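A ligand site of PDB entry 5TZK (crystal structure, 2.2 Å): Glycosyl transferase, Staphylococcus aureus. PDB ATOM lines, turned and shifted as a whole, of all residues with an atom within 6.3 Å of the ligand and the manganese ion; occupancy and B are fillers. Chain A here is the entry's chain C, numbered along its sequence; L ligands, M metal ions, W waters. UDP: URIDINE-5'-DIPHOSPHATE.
The side-chain carboxylate (OD2) of Asp 40 is in hydrogen-bond range of a nitrogen (N3) of the ligand.
An oxygen (O3') of the ligand lies within hydrogen-bond range of the backbone carbonyl oxygen (O) of Pro 8 (2.8 Å).
N of Ser 92 is in hydrogen-bond range of O3' of the ligand, 3.0 Å away.
O2' of the ligand lies within hydrogen-bond range of OG of Ser 92.
The guanidinium group (NH2) of Arg 126 is in salt-bridge range of an oxygen (O3B) of the ligand (3.4 Å).
The side-chain amide nitrogen (ND2) of Asn 67 sits at hydrogen-bond distance from an oxygen (O4) of the ligand, 3.0 Å away.
The backbone NH of Gly 70 lies within hydrogen-bond range of an oxygen (O4) of the ligand (3.2 Å).
The backbone carbonyl oxygen of Gly 70 is in hydrogen-bond range of a nitrogen (N3) of the ligand (3.5 Å).
The backbone NH (N) of Tyr 10 lies within hydrogen-bond range of an oxygen (O2') of the ligand, 3.3 Å away.
The side-chain hydroxyl (OG1) of Thr 204 is in hydrogen-bond range of the backbone carbonyl oxygen (O) of Asp 93, at 2.6 Å.
ND2 of Asn 67 lies within hydrogen-bond range of O of Asp 40, at 3.0 Å.
The side-chain hydroxyl of Ser 92 lies within hydrogen-bond range of the side-chain hydroxyl of Ser 12 (2.9 Å).
The backbone carbonyl oxygen of Gly 70 lies within hydrogen-bond range of the side-chain hydroxyl of Ser 68.
The side-chain hydroxyl (OG) of Ser 12 is in hydrogen-bond range of the backbone NH (N) of Tyr 10.
NH2 of Arg 75 is in salt-bridge range of OD1 of Asp 91.
The side-chain hydroxyl (OG1) of Thr 9 is in hydrogen-bond range of the side-chain carboxylate (OD1) of Asp 39 (2.7 Å).
OH of Tyr 15 lies within hydrogen-bond range of OG of Ser 12, 3.5 Å away.
Thr 9 touches the ligand.
Ser 12 touches the ligand.
Gly 69 touches the ligand (C to O4, 3.2 Å).
CB of Pro 71 touches O4' of the ligand, 3.1 Å away.
Pro 74 touches the ligand.
Asp 91 touches the ligand (CB to O3', 3.5 Å).
Hydrophobic or aromatic side chains within 4 Å of the ligand: Pro 8, Tyr 10, Pro 71 and Pro 74.
Of the 25 residues printed, 14 come within 4 Å of the ligand.
Merely in contact with the manganese ion: Arg 126.
O2A of the ligand binds the manganese ion (2.0 Å).
O1B of the ligand binds the manganese ion, 2.1 Å away.
Water W1 is bound to the manganese ion, 2.1 Å away.
OD2 of Asp 93 is bound to the manganese ion (2.3 Å).
Water W4 is bound to the manganese ion (2.3 Å).
OD1 of Asp 93 is bound to the manganese ion (2.4 Å).
Water W1 bridges the side-chain carboxylate (OD2) of Asp 91 (2.6 Å) and the side-chain carboxylate (OD2) of Asp 94 (3.0 Å).
Water W4 lies within hydrogen-bond range of the side-chain carboxylate (OD1) of Asp 94 (2.5 Å), the guanidinium group (NH2) of Arg 126 (3.0 Å) and the backbone NH (N) of Thr 204 (3.1 Å).
Water W3 lies within hydrogen-bond range of the side-chain hydroxyl (OH) of Tyr 15, the side-chain hydroxyl (OG) of Ser 92 and an oxygen (O1A) of the ligand.
Water W2 lies within hydrogen-bond range of the backbone carbonyl oxygen (O) of Tyr 10 (2.5 Å), the side-chain hydroxyl (OH) of Tyr 15 (2.5 Å), an oxygen (O2') of the ligand (2.9 Å) and the side-chain hydroxyl (OG) of Ser 12 (3.2 Å).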
ATOM      1  N   VAL A   7     -14.660   5.666  20.489  1.00  0.00           N
ATOM      2  CA  VAL A   7     -14.960   6.499  19.329  1.00  0.00           C
ATOM      3  C   VAL A   7     -16.360   7.066  19.424  1.00  0.00           C
ATOM      4  O   VAL A   7     -17.346   6.336  19.186  1.00  0.00           O
ATOM      5  CB  VAL A   7     -14.838   5.706  18.026  1.00  0.00           C
ATOM      6  CG1 VAL A   7     -15.058   6.651  16.826  1.00  0.00           C
ATOM      7  CG2 VAL A   7     -13.494   4.971  17.947  1.00  0.00           C
ATOM      8  N   PRO A   8     -16.502   8.361  19.715  1.00  0.00           N
ATOM      9  CA  PRO A   8     -17.829   8.996  19.624  1.00  0.00           C
ATOM     10  C   PRO A   8     -18.133   9.374  18.170  1.00  0.00           C
ATOM     11  O   PRO A   8     -17.315   9.994  17.497  1.00  0.00           O
ATOM     12  CB  PRO A   8     -17.667  10.249  20.502  1.00  0.00           C
ATOM     13  CG  PRO A   8     -16.219  10.644  20.264  1.00  0.00           C
ATOM     14  CD  PRO A   8     -15.447   9.333  20.047  1.00  0.00           C
ATOM     15  N   THR A   9     -19.314   9.000  17.682  1.00  0.00           N
ATOM     16  CA  THR A   9     -19.671   9.319  16.310  1.00  0.00           C
ATOM     17  C   THR A   9     -20.929  10.162  16.244  1.00  0.00           C
ATOM     18  O   THR A   9     -21.796  10.102  17.118  1.00  0.00           O
ATOM     19  CB  THR A   9     -19.873   8.061  15.466  1.00  0.00           C
ATOM     20  OG1 THR A   9     -20.877   7.236  16.072  1.00  0.00           O
ATOM     21  CG2 THR A   9     -18.560   7.284  15.296  1.00  0.00           C
ATOM     22  N   TYR A  10     -21.025  10.959  15.175  1.00  0.00           N
ATOM     23  CA  TYR A  10     -22.247  11.715  14.910  1.00  0.00           C
ATOM     24  C   TYR A  10     -22.246  12.113  13.439  1.00  0.00           C
ATOM     25  O   TYR A  10     -21.465  12.979  13.033  1.00  0.00           O
ATOM     26  CB  TYR A  10     -22.362  12.947  15.803  1.00  0.00           C
ATOM     27  CG  TYR A  10     -23.601  13.746  15.487  1.00  0.00           C
ATOM     28  CD1 TYR A  10     -24.867  13.169  15.544  1.00  0.00           C
ATOM     29  CD2 TYR A  10     -23.512  15.078  15.121  1.00  0.00           C
ATOM     30  CE1 TYR A  10     -26.022  13.900  15.248  1.00  0.00           C
ATOM     31  CE2 TYR A  10     -24.654  15.810  14.814  1.00  0.00           C
ATOM     32  CZ  TYR A  10     -25.913  15.224  14.878  1.00  0.00           C
ATOM     33  OH  TYR A  10     -27.018  15.975  14.573  1.00  0.00           O
ATOM     34  N   ASN A  11     -23.145  11.493  12.654  1.00  0.00           N
ATOM     35  CA  ASN A  11     -23.214  11.705  11.215  1.00  0.00           C
ATOM     36  C   ASN A  11     -21.821  11.644  10.583  1.00  0.00           C
ATOM     37  O   ASN A  11     -21.411  12.518   9.814  1.00  0.00           O
ATOM     38  CB  ASN A  11     -23.926  13.019  10.882  1.00  0.00           C
ATOM     39  CG  ASN A  11     -25.378  13.037  11.343  1.00  0.00           C
ATOM     40  OD1 ASN A  11     -26.020  11.992  11.386  1.00  0.00           O
ATOM     41  ND2 ASN A  11     -25.890  14.216  11.675  1.00  0.00           N
ATOM     42  N   SER A  12     -21.091  10.571  10.910  1.00  0.00           N
ATOM     43  CA  SER A  12     -19.715  10.375  10.484  1.00  0.00           C
ATOM     44  C   SER A  12     -19.606   9.477   9.260  1.00  0.00           C
ATOM     45  O   SER A  12     -18.540   8.924   8.987  1.00  0.00           O
ATOM     46  CB  SER A  12     -18.899   9.808  11.639  1.00  0.00           C
ATOM     47  OG  SER A  12     -19.090  10.560  12.824  1.00  0.00           O
ATOM     48  N   TYR A  15     -16.684   9.714   6.463  1.00  0.00           N
ATOM     49  CA  TYR A  15     -15.277   9.626   6.772  1.00  0.00           C
ATOM     50  C   TYR A  15     -14.927   8.557   7.809  1.00  0.00           C
ATOM     51  O   TYR A  15     -13.749   8.409   8.131  1.00  0.00           O
ATOM     52  CB  TYR A  15     -14.758  11.007   7.252  1.00  0.00           C
ATOM     53  CG  TYR A  15     -15.649  11.669   8.281  1.00  0.00           C
ATOM     54  CD1 TYR A  15     -15.612  11.265   9.614  1.00  0.00           C
ATOM     55  CD2 TYR A  15     -16.518  12.707   7.924  1.00  0.00           C
ATOM     56  CE1 TYR A  15     -16.419  11.875  10.563  1.00  0.00           C
ATOM     57  CE2 TYR A  15     -17.339  13.318   8.874  1.00  0.00           C
ATOM     58  CZ  TYR A  15     -17.283  12.892  10.200  1.00  0.00           C
ATOM     59  OH  TYR A  15     -18.068  13.471  11.181  1.00  0.00           O
ATOM     60  N   VAL A  38     -19.747   4.702  20.443  1.00  0.00           N
ATOM     61  CA  VAL A  38     -21.006   5.242  20.954  1.00  0.00           C
ATOM     62  C   VAL A  38     -21.452   6.345  20.014  1.00  0.00           C
ATOM     63  O   VAL A  38     -20.754   7.371  19.880  1.00  0.00           O
ATOM     64  CB  VAL A  38     -20.874   5.768  22.390  1.00  0.00           C
ATOM     65  CG1 VAL A  38     -22.237   6.294  22.864  1.00  0.00           C
ATOM     66  CG2 VAL A  38     -20.394   4.674  23.309  1.00  0.00           C
ATOM     67  N   ASP A  39     -22.609   6.150  19.382  1.00  0.00           N
ATOM     68  CA  ASP A  39     -23.082   7.041  18.332  1.00  0.00           C
ATOM     69  C   ASP A  39     -24.057   8.051  18.924  1.00  0.00           C
ATOM     70  O   ASP A  39     -24.980   7.665  19.652  1.00  0.00           O
ATOM     71  CB  ASP A  39     -23.740   6.241  17.218  1.00  0.00           C
ATOM     72  CG  ASP A  39     -24.273   7.130  16.130  1.00  0.00           C
ATOM     73  OD1 ASP A  39     -23.468   7.607  15.299  1.00  0.00           O
ATOM     74  OD2 ASP A  39     -25.502   7.338  16.095  1.00  0.00           O
ATOM     75  N   ASP A  40     -23.851   9.333  18.620  1.00  0.00           N
ATOM     76  CA  ASP A  40     -24.652  10.404  19.215  1.00  0.00           C
ATOM     77  C   ASP A  40     -25.963  10.634  18.458  1.00  0.00           C
ATOM     78  O   ASP A  40     -26.278  11.749  18.049  1.00  0.00           O
ATOM     79  CB  ASP A  40     -23.840  11.695  19.280  1.00  0.00           C
ATOM     80  CG  ASP A  40     -24.230  12.568  20.478  1.00  0.00           C
ATOM     81  OD1 ASP A  40     -25.269  12.284  21.115  1.00  0.00           O
ATOM     82  OD2 ASP A  40     -23.490  13.520  20.797  1.00  0.00           O
ATOM     83  N   ASN A  67     -29.504  13.220  20.577  1.00  0.00           N
ATOM     84  CA  ASN A  67     -28.176  13.765  20.354  1.00  0.00           C
ATOM     85  C   ASN A  67     -27.744  14.613  21.547  1.00  0.00           C
ATOM     86  O   ASN A  67     -28.434  15.559  21.928  1.00  0.00           O
ATOM     87  CB  ASN A  67     -28.129  14.614  19.090  1.00  0.00           C
ATOM     88  CG  ASN A  67     -26.810  15.366  18.979  1.00  0.00           C
ATOM     89  OD1 ASN A  67     -26.716  16.549  19.339  1.00  0.00           O
ATOM     90  ND2 ASN A  67     -25.758  14.657  18.535  1.00  0.00           N
ATOM     91  N   SER A  68     -26.588  14.282  22.125  1.00  0.00           N
ATOM     92  CA  SER A  68     -26.127  15.024  23.291  1.00  0.00           C
ATOM     93  C   SER A  68     -25.485  16.349  22.924  1.00  0.00           C
ATOM     94  O   SER A  68     -25.278  17.182  23.810  1.00  0.00           O
ATOM     95  CB  SER A  68     -25.140  14.178  24.098  1.00  0.00           C
ATOM     96  OG  SER A  68     -23.863  14.184  23.490  1.00  0.00           O
ATOM     97  N   GLY A  69     -25.171  16.558  21.641  1.00  0.00           N
ATOM     98  CA  GLY A  69     -24.543  17.780  21.157  1.00  0.00           C
ATOM     99  C   GLY A  69     -23.042  17.853  21.313  1.00  0.00           C
ATOM    100  O   GLY A  69     -22.466  18.917  21.052  1.00  0.00           O
ATOM    101  N   GLY A  70     -22.384  16.774  21.716  1.00  0.00           N
ATOM    102  CA  GLY A  70     -20.959  16.808  21.909  1.00  0.00           C
ATOM    103  C   GLY A  70     -20.408  15.456  22.296  1.00  0.00           C
ATOM    104  O   GLY A  70     -21.157  14.520  22.620  1.00  0.00           O
ATOM    105  N   PRO A  71     -19.081  15.313  22.278  1.00  0.00           N
ATOM    106  CA  PRO A  71     -18.471  13.998  22.494  1.00  0.00           C
ATOM    107  C   PRO A  71     -18.441  13.550  23.952  1.00  0.00           C
ATOM    108  O   PRO A  71     -18.141  12.371  24.203  1.00  0.00           O
ATOM    109  CB  PRO A  71     -17.044  14.187  21.961  1.00  0.00           C
ATOM    110  CG  PRO A  71     -16.781  15.663  22.143  1.00  0.00           C
ATOM    111  CD  PRO A  71     -18.084  16.340  21.896  1.00  0.00           C
ATOM    112  N   GLY A  72     -18.751  14.430  24.908  1.00  0.00           N
ATOM    113  CA  GLY A  72     -18.667  14.127  26.324  1.00  0.00           C
ATOM    114  C   GLY A  72     -19.473  12.927  26.795  1.00  0.00           C
ATOM    115  O   GLY A  72     -18.914  11.959  27.315  1.00  0.00           O
ATOM    116  N   PRO A  74     -21.205  10.654  24.890  1.00  0.00           N
ATOM    117  CA  PRO A  74     -20.770   9.441  24.164  1.00  0.00           C
ATOM    118  C   PRO A  74     -19.515   8.812  24.746  1.00  0.00           C
ATOM    119  O   PRO A  74     -19.489   7.598  24.978  1.00  0.00           O
ATOM    120  CB  PRO A  74     -20.546   9.957  22.746  1.00  0.00           C
ATOM    121  CG  PRO A  74     -21.506  11.082  22.602  1.00  0.00           C
ATOM    122  CD  PRO A  74     -21.588  11.745  23.954  1.00  0.00           C
ATOM    123  N   ARG A  75     -18.476   9.617  24.987  1.00  0.00           N
ATOM    124  CA  ARG A  75     -17.230   9.057  25.494  1.00  0.00           C
ATOM    125  C   ARG A  75     -17.402   8.483  26.894  1.00  0.00           C
ATOM    126  O   ARG A  75     -16.812   7.449  27.221  1.00  0.00           O
ATOM    127  CB  ARG A  75     -16.106  10.104  25.519  1.00  0.00           C
ATOM    128  CG  ARG A  75     -15.527  10.492  24.168  1.00  0.00           C
ATOM    129  CD  ARG A  75     -14.607  11.700  24.371  1.00  0.00           C
ATOM    130  NE  ARG A  75     -14.133  12.257  23.109  1.00  0.00           N
ATOM    131  CZ  ARG A  75     -13.772  13.533  22.967  1.00  0.00           C
ATOM    132  NH1 ARG A  75     -13.865  14.366  23.999  1.00  0.00           N
ATOM    133  NH2 ARG A  75     -13.347  13.966  21.782  1.00  0.00           N
ATOM    134  N   VAL A  90     -10.173   8.226  20.024  1.00  0.00           N
ATOM    135  CA  VAL A  90      -9.955   8.680  18.653  1.00  0.00           C
ATOM    136  C   VAL A  90     -11.274   9.220  18.127  1.00  0.00           C
ATOM    137  O   VAL A  90     -12.321   8.540  18.225  1.00  0.00           O
ATOM    138  CB  VAL A  90      -9.418   7.582  17.721  1.00  0.00           C
ATOM    139  CG1 VAL A  90      -8.880   8.225  16.413  1.00  0.00           C
ATOM    140  CG2 VAL A  90      -8.316   6.735  18.374  1.00  0.00           C
ATOM    141  N   ASP A  91     -11.257  10.437  17.563  1.00  0.00           N
ATOM    142  CA  ASP A  91     -12.472  11.039  17.054  1.00  0.00           C
ATOM    143  C   ASP A  91     -12.813  10.466  15.693  1.00  0.00           C
ATOM    144  O   ASP A  91     -11.945   9.982  14.967  1.00  0.00           O
ATOM    145  CB  ASP A  91     -12.351  12.568  16.959  1.00  0.00           C
ATOM    146  CG  ASP A  91     -12.366  13.259  18.323  1.00  0.00           C
ATOM    147  OD1 ASP A  91     -12.721  12.617  19.359  1.00  0.00           O
ATOM    148  OD2 ASP A  91     -12.035  14.465  18.362  1.00  0.00           O
ATOM    149  N   SER A  92     -14.096  10.573  15.328  1.00  0.00           N
ATOM    150  CA  SER A  92     -14.613   9.815  14.183  1.00  0.00           C
ATOM    151  C   SER A  92     -13.986  10.249  12.870  1.00  0.00           C
ATOM    152  O   SER A  92     -13.968   9.475  11.920  1.00  0.00           O
ATOM    153  CB  SER A  92     -16.126   9.925  14.114  1.00  0.00           C
ATOM    154  OG  SER A  92     -16.508  11.271  13.889  1.00  0.00           O
ATOM    155  N   ASP A  93     -13.457  11.474  12.807  1.00  0.00           N
ATOM    156  CA  ASP A  93     -12.869  11.986  11.578  1.00  0.00           C
ATOM    157  C   ASP A  93     -11.351  11.912  11.583  1.00  0.00           C
ATOM    158  O   ASP A  93     -10.713  12.437  10.683  1.00  0.00           O
ATOM    159  CB  ASP A  93     -13.333  13.430  11.330  1.00  0.00           C
ATOM    160  CG  ASP A  93     -12.910  14.362  12.441  1.00  0.00           C
ATOM    161  OD1 ASP A  93     -12.489  13.864  13.507  1.00  0.00           O
ATOM    162  OD2 ASP A  93     -13.036  15.588  12.282  1.00  0.00           O
ATOM    163  N   ASP A  94     -10.766  11.268  12.571  1.00  0.00           N
ATOM    164  CA  ASP A  94      -9.317  11.107  12.653  1.00  0.00           C
ATOM    165  C   ASP A  94      -8.939   9.658  12.390  1.00  0.00           C
ATOM    166  O   ASP A  94      -9.802   8.801  12.164  1.00  0.00           O
ATOM    167  CB  ASP A  94      -8.796  11.583  14.008  1.00  0.00           C
ATOM    168  CG  ASP A  94      -9.026  13.063  14.247  1.00  0.00           C
ATOM    169  OD1 ASP A  94      -9.116  13.828  13.252  1.00  0.00           O
ATOM    170  OD2 ASP A  94      -9.135  13.447  15.430  1.00  0.00           O
ATOM    171  N   ARG A 126      -4.838  21.027   9.228  1.00  0.00           N
ATOM    172  CA  ARG A 126      -5.057  21.037  10.669  1.00  0.00           C
ATOM    173  C   ARG A 126      -3.722  21.040  11.418  1.00  0.00           C
ATOM    174  O   ARG A 126      -2.743  20.428  10.982  1.00  0.00           O
ATOM    175  CB  ARG A 126      -5.905  19.820  11.067  1.00  0.00           C
ATOM    176  CG  ARG A 126      -5.959  19.482  12.547  1.00  0.00           C
ATOM    177  CD  ARG A 126      -6.806  20.471  13.321  1.00  0.00           C
ATOM    178  NE  ARG A 126      -8.204  20.076  13.390  1.00  0.00           N
ATOM    179  CZ  ARG A 126      -8.696  19.269  14.325  1.00  0.00           C
ATOM    180  NH1 ARG A 126      -7.901  18.774  15.272  1.00  0.00           N
ATOM    181  NH2 ARG A 126      -9.981  18.968  14.336  1.00  0.00           N
ATOM    182  N   THR A 204      -7.753  15.521  11.704  1.00  0.00           N
ATOM    183  CA  THR A 204      -8.398  16.124  10.535  1.00  0.00           C
ATOM    184  C   THR A 204      -8.805  17.590  10.701  1.00  0.00           C
ATOM    185  O   THR A 204      -8.795  18.360   9.720  1.00  0.00           O
ATOM    186  CB  THR A 204      -9.641  15.313  10.162  1.00  0.00           C
ATOM    187  OG1 THR A 204      -9.233  14.200   9.391  1.00  0.00           O
ATOM    188  CG2 THR A 204     -10.673  16.125   9.423  1.00  0.00           C
HETATM  189  N1  UDP L   1     -19.623  14.291  18.122  1.00  0.00           N
HETATM  190  C2  UDP L   1     -20.524  13.761  19.020  1.00  0.00           C
HETATM  191  N3  UDP L   1     -21.735  14.386  19.217  1.00  0.00           N
HETATM  192  C4  UDP L   1     -22.023  15.546  18.517  1.00  0.00           C
HETATM  193  C5  UDP L   1     -21.079  16.071  17.626  1.00  0.00           C
HETATM  194  C6  UDP L   1     -19.799  15.553  17.604  1.00  0.00           C
HETATM  195  O2  UDP L   1     -20.238  12.725  19.626  1.00  0.00           O
HETATM  196  O4  UDP L   1     -23.113  16.096  18.688  1.00  0.00           O
HETATM  197  C1' UDP L   1     -18.360  13.578  18.003  1.00  0.00           C
HETATM  198  C2' UDP L   1     -17.774  13.583  16.610  1.00  0.00           C
HETATM  199  O2' UDP L   1     -18.130  12.420  15.903  1.00  0.00           O
HETATM  200  C3' UDP L   1     -16.296  13.612  16.932  1.00  0.00           C
HETATM  201  C4' UDP L   1     -16.205  14.353  18.269  1.00  0.00           C
HETATM  202  O4' UDP L   1     -17.473  14.230  18.878  1.00  0.00           O
HETATM  203  O3' UDP L   1     -15.792  12.292  17.072  1.00  0.00           O
HETATM  204  C5' UDP L   1     -15.958  15.846  18.074  1.00  0.00           C
HETATM  205  O5' UDP L   1     -15.152  15.831  16.949  1.00  0.00           O
HETATM  206  PA  UDP L   1     -15.234  16.812  15.686  1.00  0.00           P
HETATM  207  O1A UDP L   1     -16.553  17.028  15.082  1.00  0.00           O
HETATM  208  O2A UDP L   1     -14.325  16.135  14.714  1.00  0.00           O
HETATM  209  O3A UDP L   1     -14.600  18.146  16.301  1.00  0.00           O
HETATM  210  PB  UDP L   1     -13.360  18.937  15.648  1.00  0.00           P
HETATM  211  O1B UDP L   1     -12.675  18.126  14.629  1.00  0.00           O
HETATM  212  O2B UDP L   1     -13.926  20.147  15.001  1.00  0.00           O
HETATM  213  O3B UDP L   1     -12.421  19.280  16.734  1.00  0.00           O
HETATM  214 MN    MN M   1     -12.325  16.049  14.382  1.00  0.00          MN
HETATM  215  O   HOH W   1     -11.229  15.528  16.126  1.00  0.00           O
HETATM  216  O   HOH W   2     -19.093  13.661  13.477  1.00  0.00           O
HETATM  217  O   HOH W   3     -15.896  14.302  13.212  1.00  0.00           O
HETATM  218  O   HOH W   4     -10.207  16.092  13.536  1.00  0.00           O
